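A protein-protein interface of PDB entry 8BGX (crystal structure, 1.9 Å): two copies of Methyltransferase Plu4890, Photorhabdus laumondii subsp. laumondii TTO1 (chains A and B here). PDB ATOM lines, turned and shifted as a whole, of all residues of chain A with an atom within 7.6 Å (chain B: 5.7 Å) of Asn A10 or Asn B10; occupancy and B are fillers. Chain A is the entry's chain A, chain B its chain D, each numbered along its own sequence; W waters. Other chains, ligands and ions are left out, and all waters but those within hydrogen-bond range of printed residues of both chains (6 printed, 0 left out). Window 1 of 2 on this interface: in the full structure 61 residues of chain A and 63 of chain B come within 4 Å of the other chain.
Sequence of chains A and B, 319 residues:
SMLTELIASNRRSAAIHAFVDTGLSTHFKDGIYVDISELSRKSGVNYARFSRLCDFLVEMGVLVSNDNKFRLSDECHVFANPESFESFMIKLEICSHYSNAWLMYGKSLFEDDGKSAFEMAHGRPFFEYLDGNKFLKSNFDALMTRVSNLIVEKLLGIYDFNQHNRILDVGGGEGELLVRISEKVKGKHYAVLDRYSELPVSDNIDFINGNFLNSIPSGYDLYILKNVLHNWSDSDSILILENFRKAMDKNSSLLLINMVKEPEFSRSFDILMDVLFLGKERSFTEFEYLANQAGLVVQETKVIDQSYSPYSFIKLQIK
The side-chain hydroxyl of Ser A13 is in hydrogen-bond range of the backbone NH of Ser B9, 3.1 Å away. The side-chain carboxylate of Glu A93 is in salt-bridge range of the guanidinium group of Arg B11. OG of Ser A13 lies within hydrogen-bond range of O of Ile B7. The side-chain carboxylate of Glu A93 lies close to the side-chain amide oxygen of Asn B10. N of Asn B10 lies within hydrogen-bond range of OG of Ser A13. NE of Arg A11 is in salt-bridge range of OE2 of Glu B93 (2.8 Å). OD1 of Asn A10 sits close to OE2 of Glu B93 (3.2 Å). The backbone NH (N) of Asn A10 lies within hydrogen-bond range of the side-chain hydroxyl (OG) of Ser B13. The side-chain hydroxyl (OG) of Ser B13 lies within hydrogen-bond range of the backbone carbonyl oxygen (O) of Ile A7, 2.7 Å away. The backbone NH (N) of Ser A9 is in hydrogen-bond range of the side-chain hydroxyl (OG) of Ser B13 (3.1 Å).
The backbone carbonyl oxygen (O) of Ala A8 sits close to the side-chain amide oxygen (OD1) of Asn A10, 3.5 Å away. OG of Ser B9 lies within hydrogen-bond range of O of Leu B6. NH1 of Arg A12 lies within hydrogen-bond range of O of Ala A8 (3.1 Å).
Of chain B, only Asn B10, Ser B13, Glu B93 and Ile B94 come within 4 Å of Asn A10. Of the printed residues of chain A, Trp B102 touches Arg A11 and Ala A14. Of the printed residues of chain B, Ile A94 touches Asn B10 (3.9 Å). Ser A99 touches none of the printed residues of chain B. The nearest printed residue of chain B that does not touch Leu A6 is Arg B12 (4.3 Å).
Printed residues of chain B that touch a printed residue of chain A: Leu B6, Ile B7, Ala B8, Ser B9, Asn B10, Arg B11, Arg B12, Ser B13, Ala B14, Glu B93, Ile B94 and Trp B102. Hydrophobic or aromatic side chains of chain B within 4 Å of the printed part of chain A: Leu B6, Ile B7, Ala B8, Ala B14, Ile B94 and Trp B102. Among the printed residues, 32 pairs touch across the chains.
Ser A9 touches Arg B12, and with the chains exchanged Arg A12 touches Ser B9. Asn A10 touches its own counterpart, Asn B10. Asn A10 touches Ser B13, and with the chains exchanged Ser A13 touches Asn B10.
Water W3 lies within hydrogen-bond range of O of Glu A93, ND2 of Asn B10 and NE1 of Trp A102. Water W2 bridges the backbone carbonyl oxygen of Trp B102 (2.8 Å) and a ring nitrogen (ND1) of His A17 (3.0 Å).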
ATOM      1  N   THR A   4     -27.553  -2.961 -19.010  1.00  0.00           N
ATOM      2  CA  THR A   4     -27.907  -3.914 -17.921  1.00  0.00           C
ATOM      3  C   THR A   4     -26.868  -5.042 -17.872  1.00  0.00           C
ATOM      4  O   THR A   4     -26.554  -5.484 -16.756  1.00  0.00           O
ATOM      5  CB  THR A   4     -29.348  -4.425 -18.041  1.00  0.00           C
ATOM      6  OG1 THR A   4     -29.529  -5.006 -19.331  1.00  0.00           O
ATOM      7  CG2 THR A   4     -30.356  -3.321 -17.816  1.00  0.00           C
ATOM      8  N   GLU A   5     -26.344  -5.472 -19.023  1.00  0.00           N
ATOM      9  CA  GLU A   5     -25.286  -6.517 -19.100  1.00  0.00           C
ATOM     10  C   GLU A   5     -23.962  -5.938 -18.588  1.00  0.00           C
ATOM     11  O   GLU A   5     -23.176  -6.704 -17.995  1.00  0.00           O
ATOM     12  CB  GLU A   5     -25.168  -7.078 -20.519  1.00  0.00           C
ATOM     13  CG  GLU A   5     -26.384  -7.881 -20.959  1.00  0.00           C
ATOM     14  CD  GLU A   5     -26.816  -9.005 -20.028  1.00  0.00           C
ATOM     15  OE1 GLU A   5     -25.933  -9.683 -19.462  1.00  0.00           O
ATOM     16  OE2 GLU A   5     -28.037  -9.206 -19.875  1.00  0.00           O
ATOM     17  N   LEU A   6     -23.725  -4.637 -18.779  1.00  0.00           N
ATOM     18  CA  LEU A   6     -22.552  -3.943 -18.186  1.00  0.00           C
ATOM     19  C   LEU A   6     -22.701  -3.945 -16.659  1.00  0.00           C
ATOM     20  O   LEU A   6     -21.751  -4.358 -15.981  1.00  0.00           O
ATOM     21  CB  LEU A   6     -22.430  -2.525 -18.749  1.00  0.00           C
ATOM     22  CG  LEU A   6     -21.225  -1.728 -18.248  1.00  0.00           C
ATOM     23  CD1 LEU A   6     -19.918  -2.436 -18.579  1.00  0.00           C
ATOM     24  CD2 LEU A   6     -21.233  -0.327 -18.829  1.00  0.00           C
ATOM     25  N   ILE A   7     -23.869  -3.557 -16.141  1.00  0.00           N
ATOM     26  CA  ILE A   7     -24.158  -3.556 -14.674  1.00  0.00           C
ATOM     27  C   ILE A   7     -23.922  -4.968 -14.125  1.00  0.00           C
ATOM     28  O   ILE A   7     -23.405  -5.080 -12.990  1.00  0.00           O
ATOM     29  CB  ILE A   7     -25.587  -3.057 -14.373  1.00  0.00           C
ATOM     30  CG1 ILE A   7     -25.748  -1.570 -14.699  1.00  0.00           C
ATOM     31  CG2 ILE A   7     -25.970  -3.358 -12.931  1.00  0.00           C
ATOM     32  CD1 ILE A   7     -27.184  -1.115 -14.839  1.00  0.00           C
ATOM     33  N   ALA A   8     -24.282  -5.991 -14.911  1.00  0.00           N
ATOM     34  CA  ALA A   8     -24.242  -7.426 -14.543  1.00  0.00           C
ATOM     35  C   ALA A   8     -22.949  -8.085 -15.045  1.00  0.00           C
ATOM     36  O   ALA A   8     -22.947  -9.318 -15.224  1.00  0.00           O
ATOM     37  CB  ALA A   8     -25.461  -8.126 -15.102  1.00  0.00           C
ATOM     38  N   SER A   9     -21.886  -7.306 -15.261  1.00  0.00           N
ATOM     39  CA  SER A   9     -20.549  -7.815 -15.671  1.00  0.00           C
ATOM     40  C   SER A   9     -20.099  -8.928 -14.713  1.00  0.00           C
ATOM     41  O   SER A   9     -19.553  -9.930 -15.200  1.00  0.00           O
ATOM     42  CB  SER A   9     -19.544  -6.698 -15.750  1.00  0.00           C
ATOM     43  OG  SER A   9     -19.885  -5.784 -16.781  1.00  0.00           O
ATOM     44  N   ASN A  10     -20.363  -8.778 -13.408  1.00  0.00           N
ATOM     45  CA  ASN A  10     -20.038  -9.772 -12.345  1.00  0.00           C
ATOM     46  C   ASN A  10     -20.484 -11.188 -12.748  1.00  0.00           C
ATOM     47  O   ASN A  10     -19.804 -12.152 -12.357  1.00  0.00           O
ATOM     48  CB  ASN A  10     -20.684  -9.419 -11.004  1.00  0.00           C
ATOM     49  CG  ASN A  10     -22.196  -9.391 -11.081  1.00  0.00           C
ATOM     50  OD1 ASN A  10     -22.760  -8.608 -11.840  1.00  0.00           O
ATOM     51  ND2 ASN A  10     -22.862 -10.241 -10.316  1.00  0.00           N
ATOM     52  N   ARG A  11     -21.606 -11.327 -13.459  1.00  0.00           N
ATOM     53  CA  ARG A  11     -22.174 -12.660 -13.811  1.00  0.00           C
ATOM     54  C   ARG A  11     -21.185 -13.428 -14.696  1.00  0.00           C
ATOM     55  O   ARG A  11     -21.115 -14.660 -14.550  1.00  0.00           O
ATOM     56  CB  ARG A  11     -23.540 -12.516 -14.491  1.00  0.00           C
ATOM     57  CG  ARG A  11     -24.599 -11.866 -13.614  1.00  0.00           C
ATOM     58  CD  ARG A  11     -25.915 -11.738 -14.351  1.00  0.00           C
ATOM     59  NE  ARG A  11     -26.842 -10.846 -13.675  1.00  0.00           N
ATOM     60  CZ  ARG A  11     -27.949 -10.346 -14.221  1.00  0.00           C
ATOM     61  NH1 ARG A  11     -28.711  -9.523 -13.525  1.00  0.00           N
ATOM     62  NH2 ARG A  11     -28.285 -10.659 -15.460  1.00  0.00           N
ATOM     63  N   ARG A  12     -20.447 -12.735 -15.569  1.00  0.00           N
ATOM     64  CA  ARG A  12     -19.419 -13.351 -16.455  1.00  0.00           C
ATOM     65  C   ARG A  12     -18.319 -13.974 -15.590  1.00  0.00           C
ATOM     66  O   ARG A  12     -17.960 -15.133 -15.838  1.00  0.00           O
ATOM     67  CB  ARG A  12     -18.788 -12.331 -17.410  1.00  0.00           C
ATOM     68  CG  ARG A  12     -19.619 -12.007 -18.642  1.00  0.00           C
ATOM     69  CD  ARG A  12     -20.731 -11.031 -18.342  1.00  0.00           C
ATOM     70  NE  ARG A  12     -21.676 -10.963 -19.444  1.00  0.00           N
ATOM     71  CZ  ARG A  12     -22.932 -10.534 -19.350  1.00  0.00           C
ATOM     72  NH1 ARG A  12     -23.428 -10.121 -18.191  1.00  0.00           N
ATOM     73  NH2 ARG A  12     -23.694 -10.532 -20.430  1.00  0.00           N
ATOM     74  N   SER A  13     -17.804 -13.218 -14.615  1.00  0.00           N
ATOM     75  CA  SER A  13     -16.733 -13.666 -13.688  1.00  0.00           C
ATOM     76  C   SER A  13     -17.228 -14.880 -12.890  1.00  0.00           C
ATOM     77  O   SER A  13     -16.481 -15.859 -12.780  1.00  0.00           O
ATOM     78  CB  SER A  13     -16.282 -12.542 -12.784  1.00  0.00           C
ATOM     79  OG  SER A  13     -15.634 -11.514 -13.531  1.00  0.00           O
ATOM     80  N   ALA A  14     -18.464 -14.825 -12.383  1.00  0.00           N
ATOM     81  CA  ALA A  14     -19.040 -15.851 -11.485  1.00  0.00           C
ATOM     82  C   ALA A  14     -19.265 -17.153 -12.267  1.00  0.00           C
ATOM     83  O   ALA A  14     -18.990 -18.228 -11.709  1.00  0.00           O
ATOM     84  CB  ALA A  14     -20.303 -15.324 -10.847  1.00  0.00           C
ATOM     85  N   ALA A  15     -19.710 -17.054 -13.521  1.00  0.00           N
ATOM     86  CA  ALA A  15     -19.923 -18.203 -14.435  1.00  0.00           C
ATOM     87  C   ALA A  15     -18.584 -18.906 -14.701  1.00  0.00           C
ATOM     88  O   ALA A  15     -18.533 -20.143 -14.593  1.00  0.00           O
ATOM     89  CB  ALA A  15     -20.563 -17.733 -15.716  1.00  0.00           C
ATOM     90  N   ILE A  16     -17.535 -18.145 -15.031  1.00  0.00           N
ATOM     91  CA  ILE A  16     -16.170 -18.705 -15.263  1.00  0.00           C
ATOM     92  C   ILE A  16     -15.699 -19.354 -13.959  1.00  0.00           C
ATOM     93  O   ILE A  16     -15.133 -20.453 -14.038  1.00  0.00           O
ATOM     94  CB  ILE A  16     -15.172 -17.652 -15.785  1.00  0.00           C
ATOM     95  CG1 ILE A  16     -15.579 -17.115 -17.157  1.00  0.00           C
ATOM     96  CG2 ILE A  16     -13.765 -18.229 -15.830  1.00  0.00           C
ATOM     97  CD1 ILE A  16     -14.875 -15.835 -17.552  1.00  0.00           C
ATOM     98  N   HIS A  17     -15.935 -18.715 -12.807  1.00  0.00           N
ATOM     99  CA  HIS A  17     -15.526 -19.242 -11.476  1.00  0.00           C
ATOM    100  C   HIS A  17     -16.181 -20.611 -11.238  1.00  0.00           C
ATOM    101  O   HIS A  17     -15.465 -21.538 -10.827  1.00  0.00           O
ATOM    102  CB  HIS A  17     -15.839 -18.245 -10.355  1.00  0.00           C
ATOM    103  CG  HIS A  17     -15.486 -18.759  -9.002  1.00  0.00           C
ATOM    104  ND1 HIS A  17     -16.377 -19.476  -8.231  1.00  0.00           N
ATOM    105  CD2 HIS A  17     -14.339 -18.693  -8.292  1.00  0.00           C
ATOM    106  CE1 HIS A  17     -15.799 -19.814  -7.095  1.00  0.00           C
ATOM    107  NE2 HIS A  17     -14.548 -19.346  -7.108  1.00  0.00           N
ATOM    108  N   PHE A  56     -24.043 -19.901 -21.909  1.00  0.00           N
ATOM    109  CA  PHE A  56     -23.525 -18.586 -21.446  1.00  0.00           C
ATOM    110  C   PHE A  56     -22.021 -18.502 -21.739  1.00  0.00           C
ATOM    111  O   PHE A  56     -21.563 -17.439 -22.192  1.00  0.00           O
ATOM    112  CB  PHE A  56     -23.845 -18.365 -19.966  1.00  0.00           C
ATOM    113  CG  PHE A  56     -23.510 -16.996 -19.426  1.00  0.00           C
ATOM    114  CD1 PHE A  56     -23.719 -15.849 -20.179  1.00  0.00           C
ATOM    115  CD2 PHE A  56     -23.028 -16.851 -18.136  1.00  0.00           C
ATOM    116  CE1 PHE A  56     -23.415 -14.595 -19.668  1.00  0.00           C
ATOM    117  CE2 PHE A  56     -22.735 -15.595 -17.621  1.00  0.00           C
ATOM    118  CZ  PHE A  56     -22.930 -14.468 -18.388  1.00  0.00           C
ATOM    119  N   MET A  89      -6.047 -16.773 -10.747  1.00  0.00           N
ATOM    120  CA  MET A  89      -6.672 -15.430 -10.901  1.00  0.00           C
ATOM    121  C   MET A  89      -8.177 -15.543 -10.642  1.00  0.00           C
ATOM    122  O   MET A  89      -8.721 -14.685  -9.930  1.00  0.00           O
ATOM    123  CB  MET A  89      -6.449 -14.867 -12.308  1.00  0.00           C
ATOM    124  CG  MET A  89      -6.854 -13.413 -12.443  1.00  0.00           C
ATOM    125  SD  MET A  89      -6.747 -12.815 -14.142  1.00  0.00           S
ATOM    126  CE  MET A  89      -7.506 -11.203 -13.957  1.00  0.00           C
ATOM    127  N   LEU A  92      -9.207 -16.135  -6.913  1.00  0.00           N
ATOM    128  CA  LEU A  92      -9.076 -14.930  -6.048  1.00  0.00           C
ATOM    129  C   LEU A  92     -10.068 -13.842  -6.470  1.00  0.00           C
ATOM    130  O   LEU A  92     -10.623 -13.196  -5.567  1.00  0.00           O
ATOM    131  CB  LEU A  92      -7.639 -14.406  -6.124  1.00  0.00           C
ATOM    132  CG  LEU A  92      -6.598 -15.246  -5.388  1.00  0.00           C
ATOM    133  CD1 LEU A  92      -5.195 -14.792  -5.755  1.00  0.00           C
ATOM    134  CD2 LEU A  92      -6.805 -15.179  -3.882  1.00  0.00           C
ATOM    135  N   GLU A  93     -10.270 -13.652  -7.779  1.00  0.00           N
ATOM    136  CA  GLU A  93     -10.958 -12.466  -8.358  1.00  0.00           C
ATOM    137  C   GLU A  93     -12.302 -12.228  -7.659  1.00  0.00           C
ATOM    138  O   GLU A  93     -12.597 -11.055  -7.351  1.00  0.00           O
ATOM    139  CB  GLU A  93     -11.168 -12.622  -9.866  1.00  0.00           C
ATOM    140  CG  GLU A  93     -11.640 -11.349 -10.543  1.00  0.00           C
ATOM    141  CD  GLU A  93     -10.678 -10.173 -10.457  1.00  0.00           C
ATOM    142  OE1 GLU A  93      -9.453 -10.405 -10.389  1.00  0.00           O
ATOM    143  OE2 GLU A  93     -11.155  -9.024 -10.455  1.00  0.00           O
ATOM    144  N   ILE A  94     -13.097 -13.274  -7.418  1.00  0.00           N
ATOM    145  CA  ILE A  94     -14.459 -13.098  -6.828  1.00  0.00           C
ATOM    146  C   ILE A  94     -14.584 -13.854  -5.498  1.00  0.00           C
ATOM    147  O   ILE A  94     -15.731 -14.024  -5.039  1.00  0.00           O
ATOM    148  CB  ILE A  94     -15.561 -13.487  -7.835  1.00  0.00           C
ATOM    149  CG1 ILE A  94     -15.622 -14.994  -8.093  1.00  0.00           C
ATOM    150  CG2 ILE A  94     -15.409 -12.701  -9.128  1.00  0.00           C
ATOM    151  CD1 ILE A  94     -17.003 -15.472  -8.463  1.00  0.00           C
ATOM    152  N   CYS A  95     -13.471 -14.245  -4.863  1.00  0.00           N
ATOM    153  CA  CYS A  95     -13.482 -14.825  -3.492  1.00  0.00           C
ATOM    154  C   CYS A  95     -14.146 -13.815  -2.544  1.00  0.00           C
ATOM    155  O   CYS A  95     -14.150 -12.604  -2.866  1.00  0.00           O
ATOM    156  CB  CYS A  95     -12.085 -15.210  -3.015  1.00  0.00           C
ATOM    157  SG  CYS A  95     -11.084 -13.812  -2.445  1.00  0.00           S
ATOM    158  N   TYR A  98     -12.191 -10.471  -1.548  1.00  0.00           N
ATOM    159  CA  TYR A  98     -12.100  -9.455  -2.628  1.00  0.00           C
ATOM    160  C   TYR A  98     -13.450  -8.748  -2.777  1.00  0.00           C
ATOM    161  O   TYR A  98     -13.492  -7.508  -2.843  1.00  0.00           O
ATOM    162  CB  TYR A  98     -11.675 -10.081  -3.955  1.00  0.00           C
ATOM    163  CG  TYR A  98     -10.194 -10.313  -4.111  1.00  0.00           C
ATOM    164  CD1 TYR A  98      -9.565 -10.039  -5.312  1.00  0.00           C
ATOM    165  CD2 TYR A  98      -9.422 -10.825  -3.079  1.00  0.00           C
ATOM    166  CE1 TYR A  98      -8.211 -10.266  -5.488  1.00  0.00           C
ATOM    167  CE2 TYR A  98      -8.064 -11.059  -3.238  1.00  0.00           C
ATOM    168  CZ  TYR A  98      -7.455 -10.777  -4.448  1.00  0.00           C
ATOM    169  OH  TYR A  98      -6.117 -10.996  -4.613  1.00  0.00           O
ATOM    170  N   SER A  99     -14.528  -9.531  -2.835  1.00  0.00           N
ATOM    171  CA  SER A  99     -15.926  -9.038  -2.944  1.00  0.00           C
ATOM    172  C   SER A  99     -16.211  -8.016  -1.837  1.00  0.00           C
ATOM    173  O   SER A  99     -16.688  -6.912  -2.159  1.00  0.00           O
ATOM    174  CB  SER A  99     -16.894 -10.176  -2.885  1.00  0.00           C
ATOM    175  OG  SER A  99     -18.225  -9.695  -2.846  1.00  0.00           O
ATOM    176  N   TRP A 102     -14.343  -4.858  -2.351  1.00  0.00           N
ATOM    177  CA  TRP A 102     -15.007  -4.058  -3.416  1.00  0.00           C
ATOM    178  C   TRP A 102     -16.220  -3.315  -2.839  1.00  0.00           C
ATOM    179  O   TRP A 102     -16.435  -2.150  -3.233  1.00  0.00           O
ATOM    180  CB  TRP A 102     -15.393  -4.925  -4.618  1.00  0.00           C
ATOM    181  CG  TRP A 102     -14.270  -5.140  -5.584  1.00  0.00           C
ATOM    182  CD1 TRP A 102     -13.576  -6.293  -5.786  1.00  0.00           C
ATOM    183  CD2 TRP A 102     -13.710  -4.173  -6.492  1.00  0.00           C
ATOM    184  NE1 TRP A 102     -12.623  -6.114  -6.750  1.00  0.00           N
ATOM    185  CE2 TRP A 102     -12.681  -4.826  -7.201  1.00  0.00           C
ATOM    186  CE3 TRP A 102     -13.962  -2.822  -6.765  1.00  0.00           C
ATOM    187  CZ2 TRP A 102     -11.921  -4.182  -8.175  1.00  0.00           C
ATOM    188  CZ3 TRP A 102     -13.219  -2.190  -7.737  1.00  0.00           C
ATOM    189  CH2 TRP A 102     -12.207  -2.859  -8.425  1.00  0.00           C
ATOM    190  N   LEU A 272      -8.278  -2.118  -8.853  1.00  0.00           N
ATOM    191  CA  LEU A 272      -8.060  -3.250  -7.910  1.00  0.00           C
ATOM    192  C   LEU A 272      -6.935  -2.888  -6.929  1.00  0.00           C
ATOM    193  O   LEU A 272      -7.085  -3.185  -5.731  1.00  0.00           O
ATOM    194  CB  LEU A 272      -7.724  -4.534  -8.675  1.00  0.00           C
ATOM    195  CG  LEU A 272      -7.467  -5.761  -7.799  1.00  0.00           C
ATOM    196  CD1 LEU A 272      -8.732  -6.183  -7.060  1.00  0.00           C
ATOM    197  CD2 LEU A 272      -6.928  -6.917  -8.629  1.00  0.00           C
ATOM    198  N   LEU B   6     -11.901 -10.322 -19.177  1.00  0.00           N
ATOM    199  CA  LEU B   6     -13.128 -11.157 -19.072  1.00  0.00           C
ATOM    200  C   LEU B   6     -13.195 -11.754 -17.661  1.00  0.00           C
ATOM    201  O   LEU B   6     -14.242 -11.603 -17.001  1.00  0.00           O
ATOM    202  CB  LEU B   6     -13.128 -12.249 -20.146  1.00  0.00           C
ATOM    203  CG  LEU B   6     -14.376 -13.130 -20.172  1.00  0.00           C
ATOM    204  CD1 LEU B   6     -15.634 -12.294 -20.359  1.00  0.00           C
ATOM    205  CD2 LEU B   6     -14.276 -14.187 -21.258  1.00  0.00           C
ATOM    206  N   ILE B   7     -12.105 -12.372 -17.198  1.00  0.00           N
ATOM    207  CA  ILE B   7     -11.997 -12.960 -15.828  1.00  0.00           C
ATOM    208  C   ILE B   7     -12.344 -11.879 -14.796  1.00  0.00           C
ATOM    209  O   ILE B   7     -13.024 -12.205 -13.803  1.00  0.00           O
ATOM    210  CB  ILE B   7     -10.593 -13.551 -15.594  1.00  0.00           C
ATOM    211  CG1 ILE B   7     -10.362 -14.807 -16.435  1.00  0.00           C
ATOM    212  CG2 ILE B   7     -10.352 -13.794 -14.112  1.00  0.00           C
ATOM    213  CD1 ILE B   7      -8.921 -15.274 -16.472  1.00  0.00           C
ATOM    214  N   ALA B   8     -11.903 -10.641 -15.048  1.00  0.00           N
ATOM    215  CA  ALA B   8     -12.041  -9.461 -14.162  1.00  0.00           C
ATOM    216  C   ALA B   8     -13.294  -8.642 -14.512  1.00  0.00           C
ATOM    217  O   ALA B   8     -13.323  -7.438 -14.178  1.00  0.00           O
ATOM    218  CB  ALA B   8     -10.797  -8.614 -14.276  1.00  0.00           C
ATOM    219  N   SER B   9     -14.290  -9.245 -15.165  1.00  0.00           N
ATOM    220  CA  SER B   9     -15.583  -8.583 -15.497  1.00  0.00           C
ATOM    221  C   SER B   9     -16.185  -7.957 -14.231  1.00  0.00           C
ATOM    222  O   SER B   9     -16.713  -6.832 -14.326  1.00  0.00           O
ATOM    223  CB  SER B   9     -16.542  -9.542 -16.163  1.00  0.00           C
ATOM    224  OG  SER B   9     -16.047  -9.967 -17.424  1.00  0.00           O
ATOM    225  N   ASN B  10     -16.067  -8.637 -13.084  1.00  0.00           N
ATOM    226  CA  ASN B  10     -16.577  -8.174 -11.762  1.00  0.00           C
ATOM    227  C   ASN B  10     -16.131  -6.729 -11.491  1.00  0.00           C
ATOM    228  O   ASN B  10     -16.922  -5.988 -10.901  1.00  0.00           O
ATOM    229  CB  ASN B  10     -16.128  -9.079 -10.613  1.00  0.00           C
ATOM    230  CG  ASN B  10     -14.620  -9.184 -10.528  1.00  0.00           C
ATOM    231  OD1 ASN B  10     -13.983  -9.597 -11.492  1.00  0.00           O
ATOM    232  ND2 ASN B  10     -14.042  -8.793  -9.401  1.00  0.00           N
ATOM    233  N   ARG B  11     -14.915  -6.349 -11.900  1.00  0.00           N
ATOM    234  CA  ARG B  11     -14.340  -5.000 -11.626  1.00  0.00           C
ATOM    235  C   ARG B  11     -15.239  -3.913 -12.227  1.00  0.00           C
ATOM    236  O   ARG B  11     -15.363  -2.853 -11.595  1.00  0.00           O
ATOM    237  CB  ARG B  11     -12.904  -4.893 -12.148  1.00  0.00           C
ATOM    238  CG  ARG B  11     -11.941  -5.851 -11.463  1.00  0.00           C
ATOM    239  CD  ARG B  11     -10.531  -5.739 -11.999  1.00  0.00           C
ATOM    240  NE  ARG B  11      -9.736  -6.894 -11.617  1.00  0.00           N
ATOM    241  CZ  ARG B  11      -8.535  -7.184 -12.107  1.00  0.00           C
ATOM    242  NH1 ARG B  11      -7.906  -8.274 -11.706  1.00  0.00           N
ATOM    243  NH2 ARG B  11      -7.972  -6.395 -13.005  1.00  0.00           N
ATOM    244  N   ARG B  12     -15.861  -4.171 -13.382  1.00  0.00           N
ATOM    245  CA  ARG B  12     -16.778  -3.213 -14.063  1.00  0.00           C
ATOM    246  C   ARG B  12     -17.997  -2.979 -13.167  1.00  0.00           C
ATOM    247  O   ARG B  12     -18.365  -1.809 -12.955  1.00  0.00           O
ATOM    248  CB  ARG B  12     -17.236  -3.726 -15.434  1.00  0.00           C
ATOM    249  CG  ARG B  12     -16.211  -3.568 -16.548  1.00  0.00           C
ATOM    250  CD  ARG B  12     -15.056  -4.532 -16.404  1.00  0.00           C
ATOM    251  NE  ARG B  12     -13.995  -4.261 -17.360  1.00  0.00           N
ATOM    252  CZ  ARG B  12     -12.767  -4.774 -17.302  1.00  0.00           C
ATOM    253  NH1 ARG B  12     -12.425  -5.610 -16.332  1.00  0.00           N
ATOM    254  NH2 ARG B  12     -11.884  -4.441 -18.225  1.00  0.00           N
ATOM    255  N   SER B  13     -18.590  -4.062 -12.658  1.00  0.00           N
ATOM    256  CA  SER B  13     -19.795  -4.027 -11.788  1.00  0.00           C
ATOM    257  C   SER B  13     -19.470  -3.256 -10.503  1.00  0.00           C
ATOM    258  O   SER B  13     -20.279  -2.408 -10.098  1.00  0.00           O
ATOM    259  CB  SER B  13     -20.303  -5.421 -11.492  1.00  0.00           C
ATOM    260  OG  SER B  13     -20.857  -6.022 -12.658  1.00  0.00           O
ATOM    261  N   ALA B  14     -18.315  -3.542  -9.900  1.00  0.00           N
ATOM    262  CA  ALA B  14     -17.873  -2.967  -8.610  1.00  0.00           C
ATOM    263  C   ALA B  14     -17.552  -1.478  -8.792  1.00  0.00           C
ATOM    264  O   ALA B  14     -17.837  -0.693  -7.864  1.00  0.00           O
ATOM    265  CB  ALA B  14     -16.694  -3.753  -8.081  1.00  0.00           C
ATOM    266  N   ALA B  15     -16.992  -1.101  -9.946  1.00  0.00           N
ATOM    267  CA  ALA B  15     -16.718   0.305 -10.323  1.00  0.00           C
ATOM    268  C   ALA B  15     -18.036   1.082 -10.381  1.00  0.00           C
ATOM    269  O   ALA B  15     -18.141   2.139  -9.723  1.00  0.00           O
ATOM    270  CB  ALA B  15     -15.983   0.358 -11.640  1.00  0.00           C
ATOM    271  N   GLU B  93     -26.975  -6.291  -7.292  1.00  0.00           N
ATOM    272  CA  GLU B  93     -26.201  -7.162  -8.219  1.00  0.00           C
ATOM    273  C   GLU B  93     -24.959  -7.727  -7.514  1.00  0.00           C
ATOM    274  O   GLU B  93     -24.744  -8.944  -7.629  1.00  0.00           O
ATOM    275  CB  GLU B  93     -25.814  -6.405  -9.491  1.00  0.00           C
ATOM    276  CG  GLU B  93     -25.294  -7.307 -10.598  1.00  0.00           C
ATOM    277  CD  GLU B  93     -26.270  -8.357 -11.113  1.00  0.00           C
ATOM    278  OE1 GLU B  93     -27.497  -8.112 -11.078  1.00  0.00           O
ATOM    279  OE2 GLU B  93     -25.800  -9.424 -11.545  1.00  0.00           O
ATOM    280  N   ILE B  94     -24.179  -6.897  -6.809  1.00  0.00           N
ATOM    281  CA  ILE B  94     -22.915  -7.357  -6.154  1.00  0.00           C
ATOM    282  C   ILE B  94     -23.016  -7.226  -4.628  1.00  0.00           C
ATOM    283  O   ILE B  94     -21.960  -7.313  -3.970  1.00  0.00           O
ATOM    284  CB  ILE B  94     -21.681  -6.621  -6.721  1.00  0.00           C
ATOM    285  CG1 ILE B  94     -21.648  -5.141  -6.330  1.00  0.00           C
ATOM    286  CG2 ILE B  94     -21.584  -6.813  -8.228  1.00  0.00           C
ATOM    287  CD1 ILE B  94     -20.269  -4.540  -6.384  1.00  0.00           C
ATOM    288  N   TRP B 102     -23.474 -16.665  -5.589  1.00  0.00           N
ATOM    289  CA  TRP B 102     -22.650 -16.952  -6.794  1.00  0.00           C
ATOM    290  C   TRP B 102     -21.477 -17.874  -6.432  1.00  0.00           C
ATOM    291  O   TRP B 102     -21.142 -18.737  -7.266  1.00  0.00           O
ATOM    292  CB  TRP B 102     -22.173 -15.662  -7.469  1.00  0.00           C
ATOM    293  CG  TRP B 102     -23.175 -15.071  -8.411  1.00  0.00           C
ATOM    294  CD1 TRP B 102     -23.925 -13.951  -8.208  1.00  0.00           C
ATOM    295  CD2 TRP B 102     -23.542 -15.570  -9.711  1.00  0.00           C
ATOM    296  NE1 TRP B 102     -24.726 -13.715  -9.291  1.00  0.00           N
ATOM    297  CE2 TRP B 102     -24.515 -14.688 -10.227  1.00  0.00           C
ATOM    298  CE3 TRP B 102     -23.155 -16.670 -10.488  1.00  0.00           C
ATOM    299  CZ2 TRP B 102     -25.091 -14.866 -11.483  1.00  0.00           C
ATOM    300  CZ3 TRP B 102     -23.720 -16.842 -11.732  1.00  0.00           C
ATOM    301  CH2 TRP B 102     -24.682 -15.954 -12.218  1.00  0.00           C
HETATM  302  O   HOH W   1     -22.975  -2.888 -10.971  1.00  0.00           O
HETATM  303  O   HOH W   2     -19.204 -20.441  -8.265  1.00  0.00           O
HETATM  304  O   HOH W   3     -11.677  -8.671  -7.801  1.00  0.00           O
HETATM  305  O   HOH W   4     -18.104  -1.159  -5.150  1.00  0.00           O
HETATM  306  O   HOH W   5     -25.326 -10.793  -9.275  1.00  0.00           O
HETATM  307  O   HOH W   6     -19.820  -8.389  -4.204  1.00  0.00           O
